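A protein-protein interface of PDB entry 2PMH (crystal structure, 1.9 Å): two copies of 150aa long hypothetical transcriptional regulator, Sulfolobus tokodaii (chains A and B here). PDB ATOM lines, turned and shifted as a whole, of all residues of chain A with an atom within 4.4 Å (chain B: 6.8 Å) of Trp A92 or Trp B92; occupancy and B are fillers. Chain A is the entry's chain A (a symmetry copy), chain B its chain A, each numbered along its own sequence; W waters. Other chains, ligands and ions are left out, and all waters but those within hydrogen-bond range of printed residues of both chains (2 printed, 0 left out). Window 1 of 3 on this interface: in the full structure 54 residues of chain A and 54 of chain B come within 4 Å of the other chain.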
ATOM      1  N   GLY A  90       9.599   4.367  25.134  1.00  0.00           N
ATOM      2  CA  GLY A  90      11.029   4.142  24.968  1.00  0.00           C
ATOM      3  C   GLY A  90      11.358   2.887  24.172  1.00  0.00           C
ATOM      4  O   GLY A  90      12.437   2.778  23.589  1.00  0.00           O
ATOM      5  N   VAL A  91      10.420   1.943  24.144  1.00  0.00           N
ATOM      6  CA  VAL A  91      10.602   0.684  23.415  1.00  0.00           C
ATOM      7  C   VAL A  91      10.269   0.872  21.927  1.00  0.00           C
ATOM      8  O   VAL A  91       9.125   1.178  21.583  1.00  0.00           O
ATOM      9  CB  VAL A  91       9.678  -0.435  23.998  1.00  0.00           C
ATOM     10  CG1 VAL A  91       9.741  -1.687  23.127  1.00  0.00           C
ATOM     11  CG2 VAL A  91      10.074  -0.745  25.430  1.00  0.00           C
ATOM     12  N   TRP A  92      11.253   0.699  21.043  1.00  0.00           N
ATOM     13  CA  TRP A  92      10.996   0.849  19.612  1.00  0.00           C
ATOM     14  C   TRP A  92      10.996  -0.484  18.867  1.00  0.00           C
ATOM     15  O   TRP A  92      10.519  -0.575  17.734  1.00  0.00           O
ATOM     16  CB  TRP A  92      12.006   1.802  18.961  1.00  0.00           C
ATOM     17  CG  TRP A  92      13.447   1.366  19.034  1.00  0.00           C
ATOM     18  CD1 TRP A  92      14.379   1.774  19.950  1.00  0.00           C
ATOM     19  CD2 TRP A  92      14.130   0.477  18.135  1.00  0.00           C
ATOM     20  NE1 TRP A  92      15.598   1.202  19.675  1.00  0.00           N
ATOM     21  CE2 TRP A  92      15.477   0.404  18.567  1.00  0.00           C
ATOM     22  CE3 TRP A  92      13.741  -0.265  17.009  1.00  0.00           C
ATOM     23  CZ2 TRP A  92      16.437  -0.380  17.904  1.00  0.00           C
ATOM     24  CZ3 TRP A  92      14.695  -1.045  16.352  1.00  0.00           C
ATOM     25  CH2 TRP A  92      16.030  -1.092  16.805  1.00  0.00           C
ATOM     26  N   GLY A  93      11.526  -1.522  19.504  1.00  0.00           N
ATOM     27  CA  GLY A  93      11.551  -2.816  18.852  1.00  0.00           C
ATOM     28  C   GLY A  93      11.142  -3.957  19.761  1.00  0.00           C
ATOM     29  O   GLY A  93      11.539  -4.016  20.921  1.00  0.00           O
ATOM     30  N   TYR A  95      10.510  -8.228  19.194  1.00  0.00           N
ATOM     31  CA  TYR A  95      10.538  -9.341  18.266  1.00  0.00           C
ATOM     32  C   TYR A  95      10.366 -10.633  19.043  1.00  0.00           C
ATOM     33  O   TYR A  95      10.875 -10.750  20.164  1.00  0.00           O
ATOM     34  CB  TYR A  95      11.906  -9.410  17.576  1.00  0.00           C
ATOM     35  CG  TYR A  95      12.402  -8.124  16.957  1.00  0.00           C
ATOM     36  CD1 TYR A  95      12.073  -7.783  15.643  1.00  0.00           C
ATOM     37  CD2 TYR A  95      13.229  -7.256  17.677  1.00  0.00           C
ATOM     38  CE1 TYR A  95      12.556  -6.614  15.061  1.00  0.00           C
ATOM     39  CE2 TYR A  95      13.716  -6.082  17.105  1.00  0.00           C
ATOM     40  CZ  TYR A  95      13.373  -5.768  15.794  1.00  0.00           C
ATOM     41  OH  TYR A  95      13.826  -4.602  15.219  1.00  0.00           O
ATOM     42  N   MET A 106      14.048  -3.757  22.164  1.00  0.00           N
ATOM     43  CA  MET A 106      14.995  -2.662  21.968  1.00  0.00           C
ATOM     44  C   MET A 106      14.407  -1.378  22.529  1.00  0.00           C
ATOM     45  O   MET A 106      13.292  -1.001  22.167  1.00  0.00           O
ATOM     46  CB  MET A 106      15.261  -2.438  20.479  1.00  0.00           C
ATOM     47  CG  MET A 106      15.384  -3.690  19.633  1.00  0.00           C
ATOM     48  SD  MET A 106      16.889  -4.592  19.898  1.00  0.00           S
ATOM     49  CE  MET A 106      18.038  -3.657  18.958  1.00  0.00           C
ATOM     50  N   ALA A 107      15.154  -0.691  23.386  1.00  0.00           N
ATOM     51  CA  ALA A 107      14.656   0.552  23.950  1.00  0.00           C
ATOM     52  C   ALA A 107      15.765   1.587  24.114  1.00  0.00           C
ATOM     53  O   ALA A 107      16.963   1.262  24.075  1.00  0.00           O
ATOM     54  CB  ALA A 107      13.990   0.282  25.287  1.00  0.00           C
ATOM     55  N   ARG A 108      15.362   2.841  24.292  1.00  0.00           N
ATOM     56  CA  ARG A 108      16.321   3.924  24.470  1.00  0.00           C
ATOM     57  C   ARG A 108      15.801   4.867  25.537  1.00  0.00           C
ATOM     58  O   ARG A 108      14.609   5.200  25.552  1.00  0.00           O
ATOM     59  CB  ARG A 108      16.494   4.738  23.188  1.00  0.00           C
ATOM     60  CG  ARG A 108      16.594   3.979  21.893  1.00  0.00           C
ATOM     61  CD  ARG A 108      17.123   4.941  20.830  1.00  0.00           C
ATOM     62  NE  ARG A 108      17.023   4.458  19.456  1.00  0.00           N
ATOM     63  CZ  ARG A 108      15.928   4.528  18.703  1.00  0.00           C
ATOM     64  NH1 ARG A 108      14.805   5.056  19.181  1.00  0.00           N
ATOM     65  NH2 ARG A 108      15.967   4.095  17.453  1.00  0.00           N
ATOM     66  N   LYS A 142      26.712   0.015  14.251  1.00  0.00           N
ATOM     67  CA  LYS A 142      25.895   0.350  13.086  1.00  0.00           C
ATOM     68  C   LYS A 142      24.415   0.284  13.402  1.00  0.00           C
ATOM     69  O   LYS A 142      23.968  -0.613  14.106  1.00  0.00           O
ATOM     70  CB  LYS A 142      26.210  -0.620  11.938  1.00  0.00           C
ATOM     71  CG  LYS A 142      25.447  -0.370  10.637  1.00  0.00           C
ATOM     72  CD  LYS A 142      25.762  -1.428   9.581  1.00  0.00           C
ATOM     73  CE  LYS A 142      25.131  -1.077   8.231  1.00  0.00           C
ATOM     74  NZ  LYS A 142      25.398  -2.115   7.208  1.00  0.00           N
ATOM     75  N   GLU A 143      23.651   1.250  12.901  1.00  0.00           N
ATOM     76  CA  GLU A 143      22.204   1.234  13.096  1.00  0.00           C
ATOM     77  C   GLU A 143      21.553   1.973  11.940  1.00  0.00           C
ATOM     78  O   GLU A 143      21.276   3.167  12.032  1.00  0.00           O
ATOM     79  CB  GLU A 143      21.779   1.881  14.420  1.00  0.00           C
ATOM     80  CG  GLU A 143      20.311   1.577  14.737  1.00  0.00           C
ATOM     81  CD  GLU A 143      19.812   2.228  16.007  1.00  0.00           C
ATOM     82  OE1 GLU A 143      19.518   3.439  15.971  1.00  0.00           O
ATOM     83  OE2 GLU A 143      19.704   1.528  17.041  1.00  0.00           O
ATOM     84  N   SER A 144      21.322   1.242  10.855  1.00  0.00           N
ATOM     85  CA  SER A 144      20.723   1.791   9.647  1.00  0.00           C
ATOM     86  C   SER A 144      19.558   0.900   9.224  1.00  0.00           C
ATOM     87  O   SER A 144      19.613   0.262   8.173  1.00  0.00           O
ATOM     88  CB  SER A 144      21.776   1.824   8.525  1.00  0.00           C
ATOM     89  OG  SER A 144      22.905   2.586   8.913  1.00  0.00           O
ATOM     90  N   PRO A 145      18.488   0.845  10.036  1.00  0.00           N
ATOM     91  CA  PRO A 145      17.354  -0.005   9.663  1.00  0.00           C
ATOM     92  C   PRO A 145      16.698   0.416   8.354  1.00  0.00           C
ATOM     93  O   PRO A 145      16.064  -0.400   7.682  1.00  0.00           O
ATOM     94  CB  PRO A 145      16.411   0.130  10.861  1.00  0.00           C
ATOM     95  CG  PRO A 145      16.681   1.524  11.341  1.00  0.00           C
ATOM     96  CD  PRO A 145      18.190   1.617  11.256  1.00  0.00           C
ATOM     97  N   ILE B  64      14.339 -13.049   8.883  1.00  0.00           N
ATOM     98  CA  ILE B  64      14.860 -12.019   9.772  1.00  0.00           C
ATOM     99  C   ILE B  64      15.591 -12.669  10.942  1.00  0.00           C
ATOM    100  O   ILE B  64      15.031 -13.532  11.615  1.00  0.00           O
ATOM    101  CB  ILE B  64      13.700 -11.149  10.311  1.00  0.00           C
ATOM    102  CG1 ILE B  64      12.819 -10.663   9.148  1.00  0.00           C
ATOM    103  CG2 ILE B  64      14.255  -9.990  11.129  1.00  0.00           C
ATOM    104  CD1 ILE B  64      13.574  -9.945   8.055  1.00  0.00           C
ATOM    105  N   VAL B  65      16.822 -12.235  11.197  1.00  0.00           N
ATOM    106  CA  VAL B  65      17.629 -12.816  12.254  1.00  0.00           C
ATOM    107  C   VAL B  65      18.318 -11.823  13.199  1.00  0.00           C
ATOM    108  O   VAL B  65      18.649 -10.696  12.821  1.00  0.00           O
ATOM    109  CB  VAL B  65      18.712 -13.725  11.632  1.00  0.00           C
ATOM    110  CG1 VAL B  65      18.079 -14.953  11.041  1.00  0.00           C
ATOM    111  CG2 VAL B  65      19.445 -12.972  10.523  1.00  0.00           C
ATOM    112  N   LEU B  85      31.489  -7.379  10.896  1.00  0.00           N
ATOM    113  CA  LEU B  85      30.079  -7.721  10.980  1.00  0.00           C
ATOM    114  C   LEU B  85      29.218  -6.613  10.377  1.00  0.00           C
ATOM    115  O   LEU B  85      28.195  -6.883   9.755  1.00  0.00           O
ATOM    116  CB  LEU B  85      29.678  -7.957  12.451  1.00  0.00           C
ATOM    117  CG  LEU B  85      30.240  -9.191  13.165  1.00  0.00           C
ATOM    118  CD1 LEU B  85      29.903  -9.135  14.658  1.00  0.00           C
ATOM    119  CD2 LEU B  85      29.669 -10.457  12.527  1.00  0.00           C
ATOM    120  N   ALA B  86      29.638  -5.367  10.544  1.00  0.00           N
ATOM    121  CA  ALA B  86      28.858  -4.245  10.033  1.00  0.00           C
ATOM    122  C   ALA B  86      28.868  -4.117   8.512  1.00  0.00           C
ATOM    123  O   ALA B  86      27.961  -3.517   7.936  1.00  0.00           O
ATOM    124  CB  ALA B  86      29.332  -2.941  10.671  1.00  0.00           C
ATOM    125  N   ILE B  88      28.739  -6.702   6.427  1.00  0.00           N
ATOM    126  CA  ILE B  88      28.100  -7.846   5.793  1.00  0.00           C
ATOM    127  C   ILE B  88      26.775  -7.383   5.188  1.00  0.00           C
ATOM    128  O   ILE B  88      25.958  -6.761   5.863  1.00  0.00           O
ATOM    129  CB  ILE B  88      27.822  -8.976   6.807  1.00  0.00           C
ATOM    130  CG1 ILE B  88      29.142  -9.477   7.399  1.00  0.00           C
ATOM    131  CG2 ILE B  88      27.078 -10.119   6.125  1.00  0.00           C
ATOM    132  CD1 ILE B  88      28.974 -10.618   8.373  1.00  0.00           C
ATOM    133  N   PRO B  89      26.555  -7.662   3.895  1.00  0.00           N
ATOM    134  CA  PRO B  89      25.302  -7.243   3.265  1.00  0.00           C
ATOM    135  C   PRO B  89      24.122  -7.840   4.023  1.00  0.00           C
ATOM    136  O   PRO B  89      24.160  -9.012   4.396  1.00  0.00           O
ATOM    137  CB  PRO B  89      25.416  -7.818   1.854  1.00  0.00           C
ATOM    138  CG  PRO B  89      26.904  -7.858   1.623  1.00  0.00           C
ATOM    139  CD  PRO B  89      27.404  -8.388   2.936  1.00  0.00           C
ATOM    140  N   GLY B  90      23.086  -7.039   4.249  1.00  0.00           N
ATOM    141  CA  GLY B  90      21.916  -7.522   4.969  1.00  0.00           C
ATOM    142  C   GLY B  90      21.902  -7.130   6.440  1.00  0.00           C
ATOM    143  O   GLY B  90      20.843  -7.075   7.066  1.00  0.00           O
ATOM    144  N   VAL B  91      23.083  -6.848   6.986  1.00  0.00           N
ATOM    145  CA  VAL B  91      23.217  -6.453   8.392  1.00  0.00           C
ATOM    146  C   VAL B  91      22.932  -4.953   8.559  1.00  0.00           C
ATOM    147  O   VAL B  91      23.660  -4.121   8.012  1.00  0.00           O
ATOM    148  CB  VAL B  91      24.660  -6.751   8.917  1.00  0.00           C
ATOM    149  CG1 VAL B  91      24.847  -6.179  10.320  1.00  0.00           C
ATOM    150  CG2 VAL B  91      24.925  -8.246   8.897  1.00  0.00           C
ATOM    151  N   TRP B  92      21.882  -4.599   9.301  1.00  0.00           N
ATOM    152  CA  TRP B  92      21.567  -3.186   9.510  1.00  0.00           C
ATOM    153  C   TRP B  92      21.881  -2.713  10.926  1.00  0.00           C
ATOM    154  O   TRP B  92      21.951  -1.510  11.190  1.00  0.00           O
ATOM    155  CB  TRP B  92      20.099  -2.888   9.180  1.00  0.00           C
ATOM    156  CG  TRP B  92      19.086  -3.622  10.022  1.00  0.00           C
ATOM    157  CD1 TRP B  92      18.426  -4.774   9.689  1.00  0.00           C
ATOM    158  CD2 TRP B  92      18.585  -3.231  11.312  1.00  0.00           C
ATOM    159  NE1 TRP B  92      17.544  -5.121  10.684  1.00  0.00           N
ATOM    160  CE2 TRP B  92      17.617  -4.193  11.690  1.00  0.00           C
ATOM    161  CE3 TRP B  92      18.857  -2.167  12.186  1.00  0.00           C
ATOM    162  CZ2 TRP B  92      16.916  -4.116  12.906  1.00  0.00           C
ATOM    163  CZ3 TRP B  92      18.160  -2.092  13.394  1.00  0.00           C
ATOM    164  CH2 TRP B  92      17.199  -3.064  13.739  1.00  0.00           C
ATOM    165  N   GLY B  93      22.078  -3.657  11.840  1.00  0.00           N
ATOM    166  CA  GLY B  93      22.384  -3.270  13.203  1.00  0.00           C
ATOM    167  C   GLY B  93      23.507  -4.079  13.820  1.00  0.00           C
ATOM    168  O   GLY B  93      23.577  -5.293  13.656  1.00  0.00           O
ATOM    169  N   VAL B  94      24.414  -3.395  14.508  1.00  0.00           N
ATOM    170  CA  VAL B  94      25.519  -4.054  15.199  1.00  0.00           C
ATOM    171  C   VAL B  94      25.724  -3.250  16.472  1.00  0.00           C
ATOM    172  O   VAL B  94      25.918  -2.035  16.432  1.00  0.00           O
ATOM    173  CB  VAL B  94      26.824  -4.074  14.347  1.00  0.00           C
ATOM    174  CG1 VAL B  94      27.950  -4.758  15.127  1.00  0.00           C
ATOM    175  CG2 VAL B  94      26.587  -4.825  13.051  1.00  0.00           C
ATOM    176  N   TYR B  95      25.647  -3.926  17.609  1.00  0.00           N
ATOM    177  CA  TYR B  95      25.786  -3.267  18.893  1.00  0.00           C
ATOM    178  C   TYR B  95      26.728  -4.079  19.762  1.00  0.00           C
ATOM    179  O   TYR B  95      26.714  -5.314  19.699  1.00  0.00           O
ATOM    180  CB  TYR B  95      24.430  -3.233  19.610  1.00  0.00           C
ATOM    181  CG  TYR B  95      23.268  -2.700  18.805  1.00  0.00           C
ATOM    182  CD1 TYR B  95      22.972  -1.334  18.783  1.00  0.00           C
ATOM    183  CD2 TYR B  95      22.440  -3.565  18.084  1.00  0.00           C
ATOM    184  CE1 TYR B  95      21.882  -0.846  18.068  1.00  0.00           C
ATOM    185  CE2 TYR B  95      21.348  -3.086  17.362  1.00  0.00           C
ATOM    186  CZ  TYR B  95      21.076  -1.722  17.360  1.00  0.00           C
ATOM    187  OH  TYR B  95      20.016  -1.227  16.635  1.00  0.00           O
ATOM    188  N   VAL B 105      23.803  -8.623  16.453  1.00  0.00           N
ATOM    189  CA  VAL B 105      23.722  -8.282  15.034  1.00  0.00           C
ATOM    190  C   VAL B 105      22.324  -8.490  14.439  1.00  0.00           C
ATOM    191  O   VAL B 105      21.787  -9.601  14.478  1.00  0.00           O
ATOM    192  CB  VAL B 105      24.741  -9.151  14.236  1.00  0.00           C
ATOM    193  CG1 VAL B 105      24.790  -8.730  12.763  1.00  0.00           C
ATOM    194  CG2 VAL B 105      26.109  -9.048  14.879  1.00  0.00           C
ATOM    195  N   MET B 106      21.752  -7.422  13.876  1.00  0.00           N
ATOM    196  CA  MET B 106      20.427  -7.484  13.264  1.00  0.00           C
ATOM    197  C   MET B 106      20.570  -7.555  11.753  1.00  0.00           C
ATOM    198  O   MET B 106      21.238  -6.708  11.157  1.00  0.00           O
ATOM    199  CB  MET B 106      19.619  -6.229  13.596  1.00  0.00           C
ATOM    200  CG  MET B 106      19.763  -5.704  15.010  1.00  0.00           C
ATOM    201  SD  MET B 106      18.954  -6.703  16.233  1.00  0.00           S
ATOM    202  CE  MET B 106      17.281  -6.207  16.053  1.00  0.00           C
ATOM    203  N   ALA B 107      19.931  -8.536  11.126  1.00  0.00           N
ATOM    204  CA  ALA B 107      20.017  -8.652   9.681  1.00  0.00           C
ATOM    205  C   ALA B 107      18.698  -9.114   9.068  1.00  0.00           C
ATOM    206  O   ALA B 107      17.808  -9.629   9.764  1.00  0.00           O
ATOM    207  CB  ALA B 107      21.133  -9.610   9.305  1.00  0.00           C
ATOM    208  N   ARG B 108      18.571  -8.922   7.759  1.00  0.00           N
ATOM    209  CA  ARG B 108      17.364  -9.326   7.050  1.00  0.00           C
ATOM    210  C   ARG B 108      17.759  -9.928   5.715  1.00  0.00           C
ATOM    211  O   ARG B 108      18.633  -9.393   5.022  1.00  0.00           O
ATOM    212  CB  ARG B 108      16.456  -8.132   6.760  1.00  0.00           C
ATOM    213  CG  ARG B 108      16.264  -7.124   7.860  1.00  0.00           C
ATOM    214  CD  ARG B 108      15.064  -6.254   7.489  1.00  0.00           C
ATOM    215  NE  ARG B 108      14.900  -5.050   8.299  1.00  0.00           N
ATOM    216  CZ  ARG B 108      15.551  -3.906   8.102  1.00  0.00           C
ATOM    217  NH1 ARG B 108      16.437  -3.787   7.118  1.00  0.00           N
ATOM    218  NH2 ARG B 108      15.289  -2.864   8.876  1.00  0.00           N
ATOM    219  N   LYS B 142       6.854  -5.093  17.015  1.00  0.00           N
ATOM    220  CA  LYS B 142       7.023  -3.658  16.794  1.00  0.00           C
ATOM    221  C   LYS B 142       8.408  -3.330  16.273  1.00  0.00           C
ATOM    222  O   LYS B 142       9.393  -3.903  16.721  1.00  0.00           O
ATOM    223  CB  LYS B 142       6.786  -2.902  18.110  1.00  0.00           C
ATOM    224  CG  LYS B 142       6.901  -1.380  18.024  1.00  0.00           C
ATOM    225  CD  LYS B 142       6.731  -0.719  19.391  1.00  0.00           C
ATOM    226  CE  LYS B 142       6.675   0.806  19.272  1.00  0.00           C
ATOM    227  NZ  LYS B 142       6.548   1.460  20.596  1.00  0.00           N
ATOM    228  N   GLU B 143       8.485  -2.421  15.307  1.00  0.00           N
ATOM    229  CA  GLU B 143       9.781  -1.991  14.788  1.00  0.00           C
ATOM    230  C   GLU B 143       9.642  -0.575  14.258  1.00  0.00           C
ATOM    231  O   GLU B 143       9.406  -0.368  13.069  1.00  0.00           O
ATOM    232  CB  GLU B 143      10.303  -2.905  13.673  1.00  0.00           C
ATOM    233  CG  GLU B 143      11.777  -2.618  13.369  1.00  0.00           C
ATOM    234  CD  GLU B 143      12.343  -3.452  12.243  1.00  0.00           C
ATOM    235  OE1 GLU B 143      12.073  -3.121  11.072  1.00  0.00           O
ATOM    236  OE2 GLU B 143      13.068  -4.435  12.526  1.00  0.00           O
ATOM    237  N   SER B 144       9.788   0.388  15.161  1.00  0.00           N
ATOM    238  CA  SER B 144       9.668   1.802  14.833  1.00  0.00           C
ATOM    239  C   SER B 144      10.889   2.540  15.376  1.00  0.00           C
ATOM    240  O   SER B 144      10.766   3.366  16.279  1.00  0.00           O
ATOM    241  CB  SER B 144       8.395   2.371  15.484  1.00  0.00           C
ATOM    242  OG  SER B 144       7.248   1.661  15.056  1.00  0.00           O
ATOM    243  N   PRO B 145      12.085   2.253  14.832  1.00  0.00           N
ATOM    244  CA  PRO B 145      13.278   2.939  15.332  1.00  0.00           C
ATOM    245  C   PRO B 145      13.227   4.449  15.131  1.00  0.00           C
ATOM    246  O   PRO B 145      13.886   5.198  15.854  1.00  0.00           O
ATOM    247  CB  PRO B 145      14.413   2.280  14.544  1.00  0.00           C
ATOM    248  CG  PRO B 145      13.758   1.940  13.240  1.00  0.00           C
ATOM    249  CD  PRO B 145      12.413   1.397  13.678  1.00  0.00           C
ATOM    250  N   ASN B 146      12.445   4.887  14.148  1.00  0.00           N
ATOM    251  CA  ASN B 146      12.309   6.316  13.845  1.00  0.00           C
ATOM    252  C   ASN B 146      11.700   7.109  14.988  1.00  0.00           C
ATOM    253  O   ASN B 146      11.930   8.315  15.094  1.00  0.00           O
ATOM    254  CB  ASN B 146      11.446   6.517  12.601  1.00  0.00           C
ATOM    255  CG  ASN B 146      10.071   5.887  12.743  1.00  0.00           C
ATOM    256  OD1 ASN B 146       9.951   4.674  12.902  1.00  0.00           O
ATOM    257  ND2 ASN B 146       9.030   6.705  12.680  1.00  0.00           N
ATOM    258  N   ILE B 147      10.903   6.451  15.832  1.00  0.00           N
ATOM    259  CA  ILE B 147      10.286   7.147  16.958  1.00  0.00           C
ATOM    260  C   ILE B 147      11.268   7.292  18.115  1.00  0.00           C
ATOM    261  O   ILE B 147      11.528   6.337  18.853  1.00  0.00           O
ATOM    262  CB  ILE B 147       9.027   6.419  17.479  1.00  0.00           C
ATOM    263  CG1 ILE B 147       8.058   6.134  16.323  1.00  0.00           C
ATOM    264  CG2 ILE B 147       8.349   7.270  18.534  1.00  0.00           C
ATOM    265  CD1 ILE B 147       7.696   7.361  15.512  1.00  0.00           C
ATOM    266  N   VAL B 148      11.812   8.495  18.267  1.00  0.00           N
ATOM    267  CA  VAL B 148      12.761   8.777  19.338  1.00  0.00           C
ATOM    268  C   VAL B 148      12.124   9.649  20.420  1.00  0.00           C
ATOM    269  O   VAL B 148      12.621   9.718  21.544  1.00  0.00           O
ATOM    270  CB  VAL B 148      14.028   9.481  18.790  1.00  0.00           C
ATOM    271  CG1 VAL B 148      14.801   8.529  17.877  1.00  0.00           C
ATOM    272  CG2 VAL B 148      13.631  10.742  18.027  1.00  0.00           C
ATOM    273  N   PHE B 150       8.740  10.023  22.495  1.00  0.00           N
ATOM    274  CA  PHE B 150       7.484   9.367  22.869  1.00  0.00           C
ATOM    275  C   PHE B 150       6.429  10.291  23.490  1.00  0.00           C
ATOM    276  O   PHE B 150       6.681  11.514  23.607  1.00  0.00           O
ATOM    277  CB  PHE B 150       7.778   8.191  23.817  1.00  0.00           C
ATOM    278  CG  PHE B 150       8.397   6.994  23.131  1.00  0.00           C
ATOM    279  CD1 PHE B 150       7.613   5.897  22.773  1.00  0.00           C
ATOM    280  CD2 PHE B 150       9.753   6.983  22.799  1.00  0.00           C
ATOM    281  CE1 PHE B 150       8.166   4.810  22.101  1.00  0.00           C
ATOM    282  CE2 PHE B 150      10.318   5.894  22.121  1.00  0.00           C
ATOM    283  CZ  PHE B 150       9.522   4.808  21.768  1.00  0.00           C
ATOM    284  OXT PHE B 150       5.350   9.771  23.854  1.00  0.00           O
HETATM  285  O   HOH W   1      26.009  -4.035   5.403  1.00  0.00           O
HETATM  286  O   HOH W   2      13.175   4.756  21.359  1.00  0.00           O
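The side-chain amino group (NZ) of Lys A142 sits at hydrogen-bond distance from the backbone carbonyl oxygen (O) of Val B91 (2.8 Å).
The side-chain carboxylate (OE2) of Glu B143 sits at hydrogen-bond distance from the side-chain hydroxyl (OH) of Tyr A95 (2.8 Å).
The backbone carbonyl oxygen of Ala B86 is in hydrogen-bond range of the side-chain amino group of Lys A142, 3.0 Å away.
O of Lys A142 is in hydrogen-bond range of N of Val B94.
O of Trp B92 is in hydrogen-bond range of N of Ser A144.
OH of Tyr B95 sits at hydrogen-bond distance from OE2 of Glu A143.
The guanidinium group (NH2) of Arg A108 sits at hydrogen-bond distance from the backbone carbonyl oxygen (O) of Pro B145 (2.8 Å).
The side-chain amino group of Lys B142 is in hydrogen-bond range of the backbone carbonyl oxygen of Val A91 (2.8 Å).
N of Ser B144 lies within hydrogen-bond range of O of Trp A92, at 2.8 Å.
NH2 of Arg B108 is in hydrogen-bond range of O of Pro A145 (2.8 Å).
O of Gly B90 lies within hydrogen-bond range of N of Arg B108, 3.0 Å away.
The backbone NH (N) of Trp B92 sits at hydrogen-bond distance from the backbone carbonyl oxygen (O) of Met B106 (2.9 Å).
The backbone NH of Trp A92 is in hydrogen-bond range of the backbone carbonyl oxygen of Met A106.
The side-chain carboxylate of Glu B143 lies within salt-bridge range of the guanidinium group of Arg B108.
O of Gly B93 lies within hydrogen-bond range of N of Met B106.
The side-chain carboxylate of Glu A143 is in salt-bridge range of the guanidinium group of Arg A108.
Among the printed residues, merely in contact across the chains: Gly A93 with Lys B142, Lys A142 with Gly B93, Glu A143 with Trp B92, Trp A92 with Glu B143, Gly A90 with Phe B150, Pro A145 with Pro B145, Arg A108 with Ile B147, Trp A92 with Pro B145, Pro A145 with Trp B92, Val A91 with Phe B150, Trp A92 with Lys B142, Lys A142 with Trp B92, Arg A108 with Val B148, Met A106 with Tyr B95, Tyr A95 with Met B106, Trp A92 with Trp B92, Tyr A95 with Trp B92, Trp A92 with Tyr B95 and Met A106 with Met B106.
Trp A92 touches six residues of chain B.
Of the printed residues of chain B, Lys A142 touches Ala B86, Val B91, Trp B92, Gly B93 and Val B94.
Of the printed residues of chain B, Pro A145 touches Trp B92, Arg B108 and Pro B145.
Of chain A, only Trp A92 (3.8 Å), Tyr A95 (3.9 Å), Lys A142 (3.7 Å), Glu A143 (3.4 Å), Ser A144 (2.8 Å) and Pro A145 (3.6 Å) come within 4 Å of Trp B92.
Printed residues of chain A within 4 Å of Tyr B95: Trp A92, Met A106 and Glu A143.
Of the printed residues of chain A, Ser B144 touches Trp A92 (2.8 Å).
Of the printed residues of chain A, Pro B145 touches Trp A92, Arg A108 and Pro A145.
The nearest residue of chain B that does not touch Trp A92 is Phe B150 (4.5 Å).
Hydrophobic or aromatic side chains of chain B within 4 Å of the printed part of chain A: Trp B92, Tyr B95, Met B106, Pro B145, Val B148 and Phe B150.
Printed residues of chain A that touch a printed residue of chain B: Gly A90, Val A91, Trp A92, Gly A93, Tyr A95, Met A106, Arg A108, Lys A142, Glu A143, Ser A144 and Pro A145.
Among the printed residues, 29 pairs touch across the chains.
Among the printed residues, no Asp or Glu carboxylate lies within 4 Å of a Lys or Arg side-chain nitrogen of the other chain.
Trp A92 touches Tyr B95, and with the chains exchanged Tyr A95 touches Trp B92.
Trp A92 touches Glu B143, and with the chains exchanged Glu A143 touches Trp B92.
Gly A93 touches Lys B142, and with the chains exchanged Lys A142 touches Gly B93.
Pro A145 touches its own counterpart, Pro B145.
Positions printed for both chains: 90, 91, 92, 93, 95, 106, 107, 108, 142, 143, 144 and 145.
Of the 29 pairs that touch across the chains among the printed residues, 23 have their exchanged pair printed and touching as well.
Water W1 lies within hydrogen-bond range of the side-chain amino group of Lys A142, the backbone carbonyl oxygen of Ile B88 and the backbone carbonyl oxygen of Ala B86.
Water W2 lies within hydrogen-bond range of NH1 of Arg A108 (2.7 Å), O of Gly A90 (3.1 Å) and O of Ile B147 (3.4 Å).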
